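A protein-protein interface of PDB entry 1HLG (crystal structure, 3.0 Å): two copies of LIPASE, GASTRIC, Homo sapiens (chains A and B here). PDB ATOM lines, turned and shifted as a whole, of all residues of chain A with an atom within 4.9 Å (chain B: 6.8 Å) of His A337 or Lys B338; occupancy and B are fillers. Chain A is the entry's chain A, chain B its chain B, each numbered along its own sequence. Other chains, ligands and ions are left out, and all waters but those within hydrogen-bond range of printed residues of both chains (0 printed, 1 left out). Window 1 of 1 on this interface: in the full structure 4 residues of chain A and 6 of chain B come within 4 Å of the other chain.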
ATOM      1  N   VAL A 310      20.374 -23.307  -6.650  1.00  0.00           N
ATOM      2  CA  VAL A 310      20.960 -21.982  -6.559  1.00  0.00           C
ATOM      3  C   VAL A 310      20.031 -20.854  -6.986  1.00  0.00           C
ATOM      4  O   VAL A 310      19.328 -20.965  -7.966  1.00  0.00           O
ATOM      5  CB  VAL A 310      22.234 -21.926  -7.428  1.00  0.00           C
ATOM      6  CG1 VAL A 310      22.957 -20.649  -7.242  1.00  0.00           C
ATOM      7  CG2 VAL A 310      23.110 -23.063  -7.078  1.00  0.00           C
ATOM      8  N   ASN A 312      20.496 -16.705  -7.551  1.00  0.00           N
ATOM      9  CA  ASN A 312      21.449 -15.590  -7.551  1.00  0.00           C
ATOM     10  C   ASN A 312      20.826 -14.278  -8.054  1.00  0.00           C
ATOM     11  O   ASN A 312      19.808 -14.268  -8.742  1.00  0.00           O
ATOM     12  CB  ASN A 312      22.702 -15.970  -8.353  1.00  0.00           C
ATOM     13  CG  ASN A 312      22.421 -16.213  -9.794  1.00  0.00           C
ATOM     14  OD1 ASN A 312      21.512 -16.939 -10.162  1.00  0.00           O
ATOM     15  ND2 ASN A 312      23.220 -15.605 -10.631  1.00  0.00           N
ATOM     16  N   LEU A 328      28.293 -22.444 -11.598  1.00  0.00           N
ATOM     17  CA  LEU A 328      27.234 -23.385 -11.976  1.00  0.00           C
ATOM     18  C   LEU A 328      27.667 -24.624 -12.784  1.00  0.00           C
ATOM     19  O   LEU A 328      27.345 -25.760 -12.425  1.00  0.00           O
ATOM     20  CB  LEU A 328      26.110 -22.623 -12.692  1.00  0.00           C
ATOM     21  CG  LEU A 328      25.404 -21.515 -11.880  1.00  0.00           C
ATOM     22  CD1 LEU A 328      24.313 -20.940 -12.700  1.00  0.00           C
ATOM     23  CD2 LEU A 328      24.766 -22.050 -10.627  1.00  0.00           C
ATOM     24  N   LEU A 334      23.697 -30.206  -9.917  1.00  0.00           N
ATOM     25  CA  LEU A 334      22.951 -28.974  -9.696  1.00  0.00           C
ATOM     26  C   LEU A 334      21.487 -29.249 -10.080  1.00  0.00           C
ATOM     27  O   LEU A 334      21.140 -29.351 -11.267  1.00  0.00           O
ATOM     28  CB  LEU A 334      23.527 -27.861 -10.559  1.00  0.00           C
ATOM     29  CG  LEU A 334      22.739 -26.566 -10.690  1.00  0.00           C
ATOM     30  CD1 LEU A 334      22.355 -25.963  -9.364  1.00  0.00           C
ATOM     31  CD2 LEU A 334      23.606 -25.629 -11.435  1.00  0.00           C
ATOM     32  N   ILE A 335      20.619 -29.362  -9.084  1.00  0.00           N
ATOM     33  CA  ILE A 335      19.224 -29.680  -9.361  1.00  0.00           C
ATOM     34  C   ILE A 335      18.271 -28.538  -9.706  1.00  0.00           C
ATOM     35  O   ILE A 335      17.127 -28.786 -10.105  1.00  0.00           O
ATOM     36  CB  ILE A 335      18.624 -30.441  -8.200  1.00  0.00           C
ATOM     37  CG1 ILE A 335      18.346 -29.483  -7.047  1.00  0.00           C
ATOM     38  CG2 ILE A 335      19.578 -31.519  -7.775  1.00  0.00           C
ATOM     39  CD1 ILE A 335      17.574 -30.027  -5.937  1.00  0.00           C
ATOM     40  N   TYR A 336      18.717 -27.293  -9.563  1.00  0.00           N
ATOM     41  CA  TYR A 336      17.861 -26.147  -9.882  1.00  0.00           C
ATOM     42  C   TYR A 336      18.632 -24.853  -9.917  1.00  0.00           C
ATOM     43  O   TYR A 336      19.656 -24.714  -9.261  1.00  0.00           O
ATOM     44  CB  TYR A 336      16.764 -26.004  -8.859  1.00  0.00           C
ATOM     45  CG  TYR A 336      15.874 -24.809  -9.078  1.00  0.00           C
ATOM     46  CD1 TYR A 336      14.857 -24.837 -10.021  1.00  0.00           C
ATOM     47  CD2 TYR A 336      16.001 -23.671  -8.300  1.00  0.00           C
ATOM     48  CE1 TYR A 336      13.960 -23.745 -10.185  1.00  0.00           C
ATOM     49  CE2 TYR A 336      15.121 -22.570  -8.453  1.00  0.00           C
ATOM     50  CZ  TYR A 336      14.096 -22.614  -9.392  1.00  0.00           C
ATOM     51  OH  TYR A 336      13.204 -21.547  -9.498  1.00  0.00           O
ATOM     52  N   HIS A 337      18.145 -23.897 -10.690  1.00  0.00           N
ATOM     53  CA  HIS A 337      18.818 -22.602 -10.775  1.00  0.00           C
ATOM     54  C   HIS A 337      17.883 -21.496 -11.236  1.00  0.00           C
ATOM     55  O   HIS A 337      17.200 -21.649 -12.228  1.00  0.00           O
ATOM     56  CB  HIS A 337      19.994 -22.635 -11.745  1.00  0.00           C
ATOM     57  CG  HIS A 337      20.615 -21.298 -11.962  1.00  0.00           C
ATOM     58  ND1 HIS A 337      21.262 -20.955 -13.130  1.00  0.00           N
ATOM     59  CD2 HIS A 337      20.672 -20.202 -11.164  1.00  0.00           C
ATOM     60  CE1 HIS A 337      21.689 -19.705 -13.041  1.00  0.00           C
ATOM     61  NE2 HIS A 337      21.348 -19.224 -11.862  1.00  0.00           N
ATOM     62  N   LYS A 338      17.870 -20.389 -10.516  1.00  0.00           N
ATOM     63  CA  LYS A 338      17.048 -19.274 -10.888  1.00  0.00           C
ATOM     64  C   LYS A 338      17.802 -17.987 -10.603  1.00  0.00           C
ATOM     65  O   LYS A 338      18.418 -17.847  -9.552  1.00  0.00           O
ATOM     66  CB  LYS A 338      15.730 -19.261 -10.122  1.00  0.00           C
ATOM     67  CG  LYS A 338      14.809 -18.073 -10.503  1.00  0.00           C
ATOM     68  CD  LYS A 338      13.593 -17.954  -9.568  1.00  0.00           C
ATOM     69  CE  LYS A 338      12.696 -16.772  -9.916  1.00  0.00           C
ATOM     70  NZ  LYS A 338      11.439 -16.793  -9.096  1.00  0.00           N
ATOM     71  N   GLU A 339      17.774 -17.052 -11.552  1.00  0.00           N
ATOM     72  CA  GLU A 339      18.428 -15.766 -11.360  1.00  0.00           C
ATOM     73  C   GLU A 339      17.411 -14.615 -11.288  1.00  0.00           C
ATOM     74  O   GLU A 339      16.792 -14.265 -12.285  1.00  0.00           O
ATOM     75  CB  GLU A 339      19.423 -15.499 -12.475  1.00  0.00           C
ATOM     76  CG  GLU A 339      20.168 -14.206 -12.249  1.00  0.00           C
ATOM     77  CD  GLU A 339      21.201 -13.898 -13.316  1.00  0.00           C
ATOM     78  OE1 GLU A 339      21.904 -14.843 -13.791  1.00  0.00           O
ATOM     79  OE2 GLU A 339      21.326 -12.695 -13.651  1.00  0.00           O
ATOM     80  N   ALA B 309       3.248 -22.183 -17.248  1.00  0.00           N
ATOM     81  CA  ALA B 309       4.542 -21.884 -16.654  1.00  0.00           C
ATOM     82  C   ALA B 309       5.332 -21.239 -17.784  1.00  0.00           C
ATOM     83  O   ALA B 309       5.311 -21.729 -18.899  1.00  0.00           O
ATOM     84  CB  ALA B 309       5.225 -23.169 -16.173  1.00  0.00           C
ATOM     85  N   VAL B 310       6.028 -20.146 -17.508  1.00  0.00           N
ATOM     86  CA  VAL B 310       6.756 -19.475 -18.565  1.00  0.00           C
ATOM     87  C   VAL B 310       8.239 -19.342 -18.291  1.00  0.00           C
ATOM     88  O   VAL B 310       8.637 -19.055 -17.179  1.00  0.00           O
ATOM     89  CB  VAL B 310       6.189 -18.050 -18.797  1.00  0.00           C
ATOM     90  CG1 VAL B 310       6.839 -17.406 -19.996  1.00  0.00           C
ATOM     91  CG2 VAL B 310       4.704 -18.098 -18.973  1.00  0.00           C
ATOM     92  N   TRP B 311       9.039 -19.557 -19.332  1.00  0.00           N
ATOM     93  CA  TRP B 311      10.493 -19.407 -19.305  1.00  0.00           C
ATOM     94  C   TRP B 311      10.830 -18.504 -20.506  1.00  0.00           C
ATOM     95  O   TRP B 311      10.543 -18.872 -21.643  1.00  0.00           O
ATOM     96  CB  TRP B 311      11.198 -20.747 -19.512  1.00  0.00           C
ATOM     97  CG  TRP B 311      11.165 -21.704 -18.374  1.00  0.00           C
ATOM     98  CD1 TRP B 311      12.208 -22.045 -17.572  1.00  0.00           C
ATOM     99  CD2 TRP B 311      10.063 -22.540 -17.983  1.00  0.00           C
ATOM    100  NE1 TRP B 311      11.836 -23.054 -16.706  1.00  0.00           N
ATOM    101  CE2 TRP B 311      10.525 -23.377 -16.940  1.00  0.00           C
ATOM    102  CE3 TRP B 311       8.739 -22.666 -18.416  1.00  0.00           C
ATOM    103  CZ2 TRP B 311       9.712 -24.328 -16.323  1.00  0.00           C
ATOM    104  CZ3 TRP B 311       7.933 -23.609 -17.806  1.00  0.00           C
ATOM    105  CH2 TRP B 311       8.420 -24.428 -16.772  1.00  0.00           C
ATOM    106  N   ASN B 312      11.423 -17.336 -20.275  1.00  0.00           N
ATOM    107  CA  ASN B 312      11.768 -16.448 -21.380  1.00  0.00           C
ATOM    108  C   ASN B 312      13.223 -15.996 -21.338  1.00  0.00           C
ATOM    109  O   ASN B 312      13.860 -16.032 -20.310  1.00  0.00           O
ATOM    110  CB  ASN B 312      10.818 -15.255 -21.393  1.00  0.00           C
ATOM    111  CG  ASN B 312      10.950 -14.387 -20.169  1.00  0.00           C
ATOM    112  OD1 ASN B 312      10.751 -14.828 -19.036  1.00  0.00           O
ATOM    113  ND2 ASN B 312      11.287 -13.124 -20.397  1.00  0.00           N
ATOM    114  N   GLY B 313      13.761 -15.572 -22.461  1.00  0.00           N
ATOM    115  CA  GLY B 313      15.153 -15.167 -22.457  1.00  0.00           C
ATOM    116  C   GLY B 313      15.376 -13.673 -22.378  1.00  0.00           C
ATOM    117  O   GLY B 313      14.571 -12.873 -22.880  1.00  0.00           O
ATOM    118  N   TYR B 336       3.934 -20.098 -12.766  1.00  0.00           N
ATOM    119  CA  TYR B 336       5.390 -20.054 -12.635  1.00  0.00           C
ATOM    120  C   TYR B 336       6.024 -19.165 -13.699  1.00  0.00           C
ATOM    121  O   TYR B 336       5.497 -19.059 -14.805  1.00  0.00           O
ATOM    122  CB  TYR B 336       5.943 -21.468 -12.774  1.00  0.00           C
ATOM    123  CG  TYR B 336       7.440 -21.568 -12.631  1.00  0.00           C
ATOM    124  CD1 TYR B 336       8.034 -21.772 -11.387  1.00  0.00           C
ATOM    125  CD2 TYR B 336       8.268 -21.493 -13.745  1.00  0.00           C
ATOM    126  CE1 TYR B 336       9.435 -21.905 -11.249  1.00  0.00           C
ATOM    127  CE2 TYR B 336       9.673 -21.618 -13.627  1.00  0.00           C
ATOM    128  CZ  TYR B 336      10.251 -21.827 -12.371  1.00  0.00           C
ATOM    129  OH  TYR B 336      11.626 -21.942 -12.227  1.00  0.00           O
ATOM    130  N   HIS B 337       7.139 -18.510 -13.371  1.00  0.00           N
ATOM    131  CA  HIS B 337       7.829 -17.684 -14.350  1.00  0.00           C
ATOM    132  C   HIS B 337       9.290 -17.555 -13.997  1.00  0.00           C
ATOM    133  O   HIS B 337       9.635 -17.326 -12.847  1.00  0.00           O
ATOM    134  CB  HIS B 337       7.228 -16.286 -14.485  1.00  0.00           C
ATOM    135  CG  HIS B 337       8.089 -15.355 -15.273  1.00  0.00           C
ATOM    136  ND1 HIS B 337       8.603 -14.186 -14.746  1.00  0.00           N
ATOM    137  CD2 HIS B 337       8.668 -15.493 -16.494  1.00  0.00           C
ATOM    138  CE1 HIS B 337       9.465 -13.651 -15.599  1.00  0.00           C
ATOM    139  NE2 HIS B 337       9.526 -14.426 -16.671  1.00  0.00           N
ATOM    140  N   LYS B 338      10.144 -17.709 -14.994  1.00  0.00           N
ATOM    141  CA  LYS B 338      11.567 -17.605 -14.776  1.00  0.00           C
ATOM    142  C   LYS B 338      12.208 -16.940 -15.991  1.00  0.00           C
ATOM    143  O   LYS B 338      11.891 -17.286 -17.124  1.00  0.00           O
ATOM    144  CB  LYS B 338      12.129 -19.002 -14.544  1.00  0.00           C
ATOM    145  CG  LYS B 338      13.625 -19.064 -14.282  1.00  0.00           C
ATOM    146  CD  LYS B 338      14.031 -20.480 -13.890  1.00  0.00           C
ATOM    147  CE  LYS B 338      15.449 -20.823 -14.330  1.00  0.00           C
ATOM    148  NZ  LYS B 338      15.629 -22.308 -14.289  1.00  0.00           N
ATOM    149  N   GLU B 339      13.094 -15.977 -15.780  1.00  0.00           N
ATOM    150  CA  GLU B 339      13.707 -15.334 -16.925  1.00  0.00           C
ATOM    151  C   GLU B 339      15.223 -15.581 -16.999  1.00  0.00           C
ATOM    152  O   GLU B 339      15.992 -15.050 -16.218  1.00  0.00           O
ATOM    153  CB  GLU B 339      13.404 -13.839 -16.892  1.00  0.00           C
ATOM    154  CG  GLU B 339      14.112 -13.122 -18.017  1.00  0.00           C
ATOM    155  CD  GLU B 339      14.402 -11.698 -17.702  1.00  0.00           C
ATOM    156  OE1 GLU B 339      13.425 -11.001 -17.327  1.00  0.00           O
ATOM    157  OE2 GLU B 339      15.603 -11.306 -17.833  1.00  0.00           O
ATOM    158  N   ILE B 340      15.655 -16.393 -17.939  1.00  0.00           N
ATOM    159  CA  ILE B 340      17.071 -16.670 -18.054  1.00  0.00           C
ATOM    160  C   ILE B 340      17.709 -15.517 -18.818  1.00  0.00           C
ATOM    161  O   ILE B 340      17.569 -15.419 -20.027  1.00  0.00           O
ATOM    162  CB  ILE B 340      17.265 -18.004 -18.797  1.00  0.00           C
ATOM    163  CG1 ILE B 340      16.358 -19.040 -18.121  1.00  0.00           C
ATOM    164  CG2 ILE B 340      18.765 -18.416 -18.860  1.00  0.00           C
ATOM    165  CD1 ILE B 340      16.352 -20.373 -18.785  1.00  0.00           C
ATOM    166  N   PRO B 341      18.440 -14.626 -18.111  1.00  0.00           N
ATOM    167  CA  PRO B 341      19.103 -13.462 -18.697  1.00  0.00           C
ATOM    168  C   PRO B 341      19.971 -13.682 -19.943  1.00  0.00           C
ATOM    169  O   PRO B 341      19.807 -12.958 -20.921  1.00  0.00           O
ATOM    170  CB  PRO B 341      19.920 -12.938 -17.526  1.00  0.00           C
ATOM    171  CG  PRO B 341      20.316 -14.213 -16.819  1.00  0.00           C
ATOM    172  CD  PRO B 341      18.959 -14.869 -16.756  1.00  0.00           C
ATOM    173  N   PHE B 348      16.608 -22.062 -25.799  1.00  0.00           N
ATOM    174  CA  PHE B 348      15.631 -22.932 -25.160  1.00  0.00           C
ATOM    175  C   PHE B 348      15.565 -24.317 -25.683  1.00  0.00           C
ATOM    176  O   PHE B 348      15.019 -25.238 -25.043  1.00  0.00           O
ATOM    177  CB  PHE B 348      14.247 -22.319 -25.217  1.00  0.00           C
ATOM    178  CG  PHE B 348      14.105 -21.152 -24.305  1.00  0.00           C
ATOM    179  CD1 PHE B 348      14.463 -19.872 -24.718  1.00  0.00           C
ATOM    180  CD2 PHE B 348      13.692 -21.345 -22.996  1.00  0.00           C
ATOM    181  CE1 PHE B 348      14.407 -18.803 -23.836  1.00  0.00           C
ATOM    182  CE2 PHE B 348      13.632 -20.282 -22.102  1.00  0.00           C
ATOM    183  CZ  PHE B 348      13.992 -19.008 -22.521  1.00  0.00           C
ATOM    184  N   ASP B 353      23.187 -25.917 -21.595  1.00  0.00           N
ATOM    185  CA  ASP B 353      22.754 -25.979 -20.215  1.00  0.00           C
ATOM    186  C   ASP B 353      21.228 -25.878 -20.120  1.00  0.00           C
ATOM    187  O   ASP B 353      20.675 -25.555 -19.063  1.00  0.00           O
ATOM    188  CB  ASP B 353      23.445 -24.875 -19.384  1.00  0.00           C
ATOM    189  CG  ASP B 353      23.278 -23.489 -19.968  1.00  0.00           C
ATOM    190  OD1 ASP B 353      22.842 -23.363 -21.128  1.00  0.00           O
ATOM    191  OD2 ASP B 353      23.596 -22.513 -19.259  1.00  0.00           O
ATOM    192  N   GLN B 356      19.705 -27.918 -17.138  1.00  0.00           N
ATOM    193  CA  GLN B 356      19.886 -27.246 -15.834  1.00  0.00           C
ATOM    194  C   GLN B 356      19.037 -25.971 -15.717  1.00  0.00           C
ATOM    195  O   GLN B 356      18.509 -25.642 -14.627  1.00  0.00           O
ATOM    196  CB  GLN B 356      21.357 -26.841 -15.590  1.00  0.00           C
ATOM    197  CG  GLN B 356      22.326 -28.010 -15.419  1.00  0.00           C
ATOM    198  CD  GLN B 356      22.624 -28.764 -16.743  1.00  0.00           C
ATOM    199  OE1 GLN B 356      21.793 -29.527 -17.252  1.00  0.00           O
ATOM    200  NE2 GLN B 356      23.824 -28.538 -17.301  1.00  0.00           N
ATOM    201  N   GLU B 357      18.906 -25.250 -16.832  1.00  0.00           N
ATOM    202  CA  GLU B 357      18.125 -24.003 -16.847  1.00  0.00           C
ATOM    203  C   GLU B 357      16.621 -24.141 -17.067  1.00  0.00           C
ATOM    204  O   GLU B 357      15.848 -23.379 -16.483  1.00  0.00           O
ATOM    205  CB  GLU B 357      18.703 -23.038 -17.886  1.00  0.00           C
ATOM    206  CG  GLU B 357      20.082 -22.555 -17.508  1.00  0.00           C
ATOM    207  CD  GLU B 357      20.071 -21.477 -16.422  1.00  0.00           C
ATOM    208  OE1 GLU B 357      19.424 -21.661 -15.382  1.00  0.00           O
ATOM    209  OE2 GLU B 357      20.727 -20.433 -16.608  1.00  0.00           O
ATOM    210  N   VAL B 358      16.205 -25.113 -17.877  1.00  0.00           N
ATOM    211  CA  VAL B 358      14.790 -25.284 -18.172  1.00  0.00           C
ATOM    212  C   VAL B 358      14.238 -26.685 -17.994  1.00  0.00           C
ATOM    213  O   VAL B 358      13.328 -26.929 -17.185  1.00  0.00           O
ATOM    214  CB  VAL B 358      14.461 -24.880 -19.648  1.00  0.00           C
ATOM    215  CG1 VAL B 358      12.957 -24.876 -19.879  1.00  0.00           C
ATOM    216  CG2 VAL B 358      15.042 -23.531 -19.970  1.00  0.00           C
ATOM    217  N   ASP B 361      13.469 -28.382 -14.514  1.00  0.00           N
ATOM    218  CA  ASP B 361      12.315 -27.757 -13.867  1.00  0.00           C
ATOM    219  C   ASP B 361      10.988 -28.333 -14.379  1.00  0.00           C
ATOM    220  O   ASP B 361      10.021 -28.513 -13.613  1.00  0.00           O
ATOM    221  CB  ASP B 361      12.286 -26.235 -14.145  1.00  0.00           C
ATOM    222  CG  ASP B 361      13.559 -25.505 -13.718  1.00  0.00           C
ATOM    223  OD1 ASP B 361      14.612 -26.145 -13.481  1.00  0.00           O
ATOM    224  OD2 ASP B 361      13.506 -24.260 -13.651  1.00  0.00           O
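OH of Tyr B336 sits at hydrogen-bond distance from OH of Tyr A336 (3.2 Å).
The backbone carbonyl oxygen (O) of His A337 is in hydrogen-bond range of the side-chain amino group (NZ) of Lys B338, 2.7 Å away.
ND1 of His A337 lies within hydrogen-bond range of OE1 of Glu B357.
The backbone NH (N) of Val A310 is in hydrogen-bond range of the backbone carbonyl oxygen (O) of Tyr A336.
The side-chain amide oxygen of Asn A312 sits at hydrogen-bond distance from a ring nitrogen (NE2) of His A337 (2.9 Å).
The backbone NH (N) of Val B310 lies within hydrogen-bond range of the backbone carbonyl oxygen (O) of Tyr B336 (3.0 Å).
O of Lys B338 lies within hydrogen-bond range of N of Asn B312 (3.2 Å).
The side-chain amino group (NZ) of Lys B338 is in hydrogen-bond range of the backbone carbonyl oxygen (O) of Glu B357 (2.5 Å).
NZ of Lys B338 lies within salt-bridge range of OD2 of Asp B361, 3.0 Å away.
Among the printed residues, pairs that only touch across the chains: Glu A339 with Pro B341 and Tyr A336 with Asp B361.
His A337 touches just these residues of chain B: Lys B338 and Glu B357.
Printed residues of chain A within 4 Å of Lys B338: His A337 (2.7 Å).
Printed residues of chain B within 4 Å of Glu A339: Pro B341.
Printed residues of chain A within 4 Å of Tyr B336: Tyr A336 (3.2 Å).
Of the printed residues of chain A, Asp B361 touches Tyr A336 (3.5 Å).
Of the printed residues of chain A, Glu B357 touches His A337.
The nearest residue of chain B that does not touch His A337 is Gln B356 (4.3 Å).
The nearest residue of chain A that does not touch Lys B338 is Lys A338 (4.1 Å).
Printed residues of chain A that touch a printed residue of chain B: Tyr A336, His A337 and Glu A339.
Hydrophobic or aromatic side chains of chain A that line the printed part of chain B: Tyr A336 and His A337.
Of the 17 printed residues of chain B, 5 touch a printed residue of chain A.
Printed residues of chain B that touch a printed residue of chain A: Tyr B336, Lys B338, Pro B341, Glu B357 and Asp B361.
Tyr A336 touches its own counterpart, Tyr B336.
His A337 touches Lys B338, but with the chains exchanged Lys A338 does not touch His B337 (4.2 Å).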
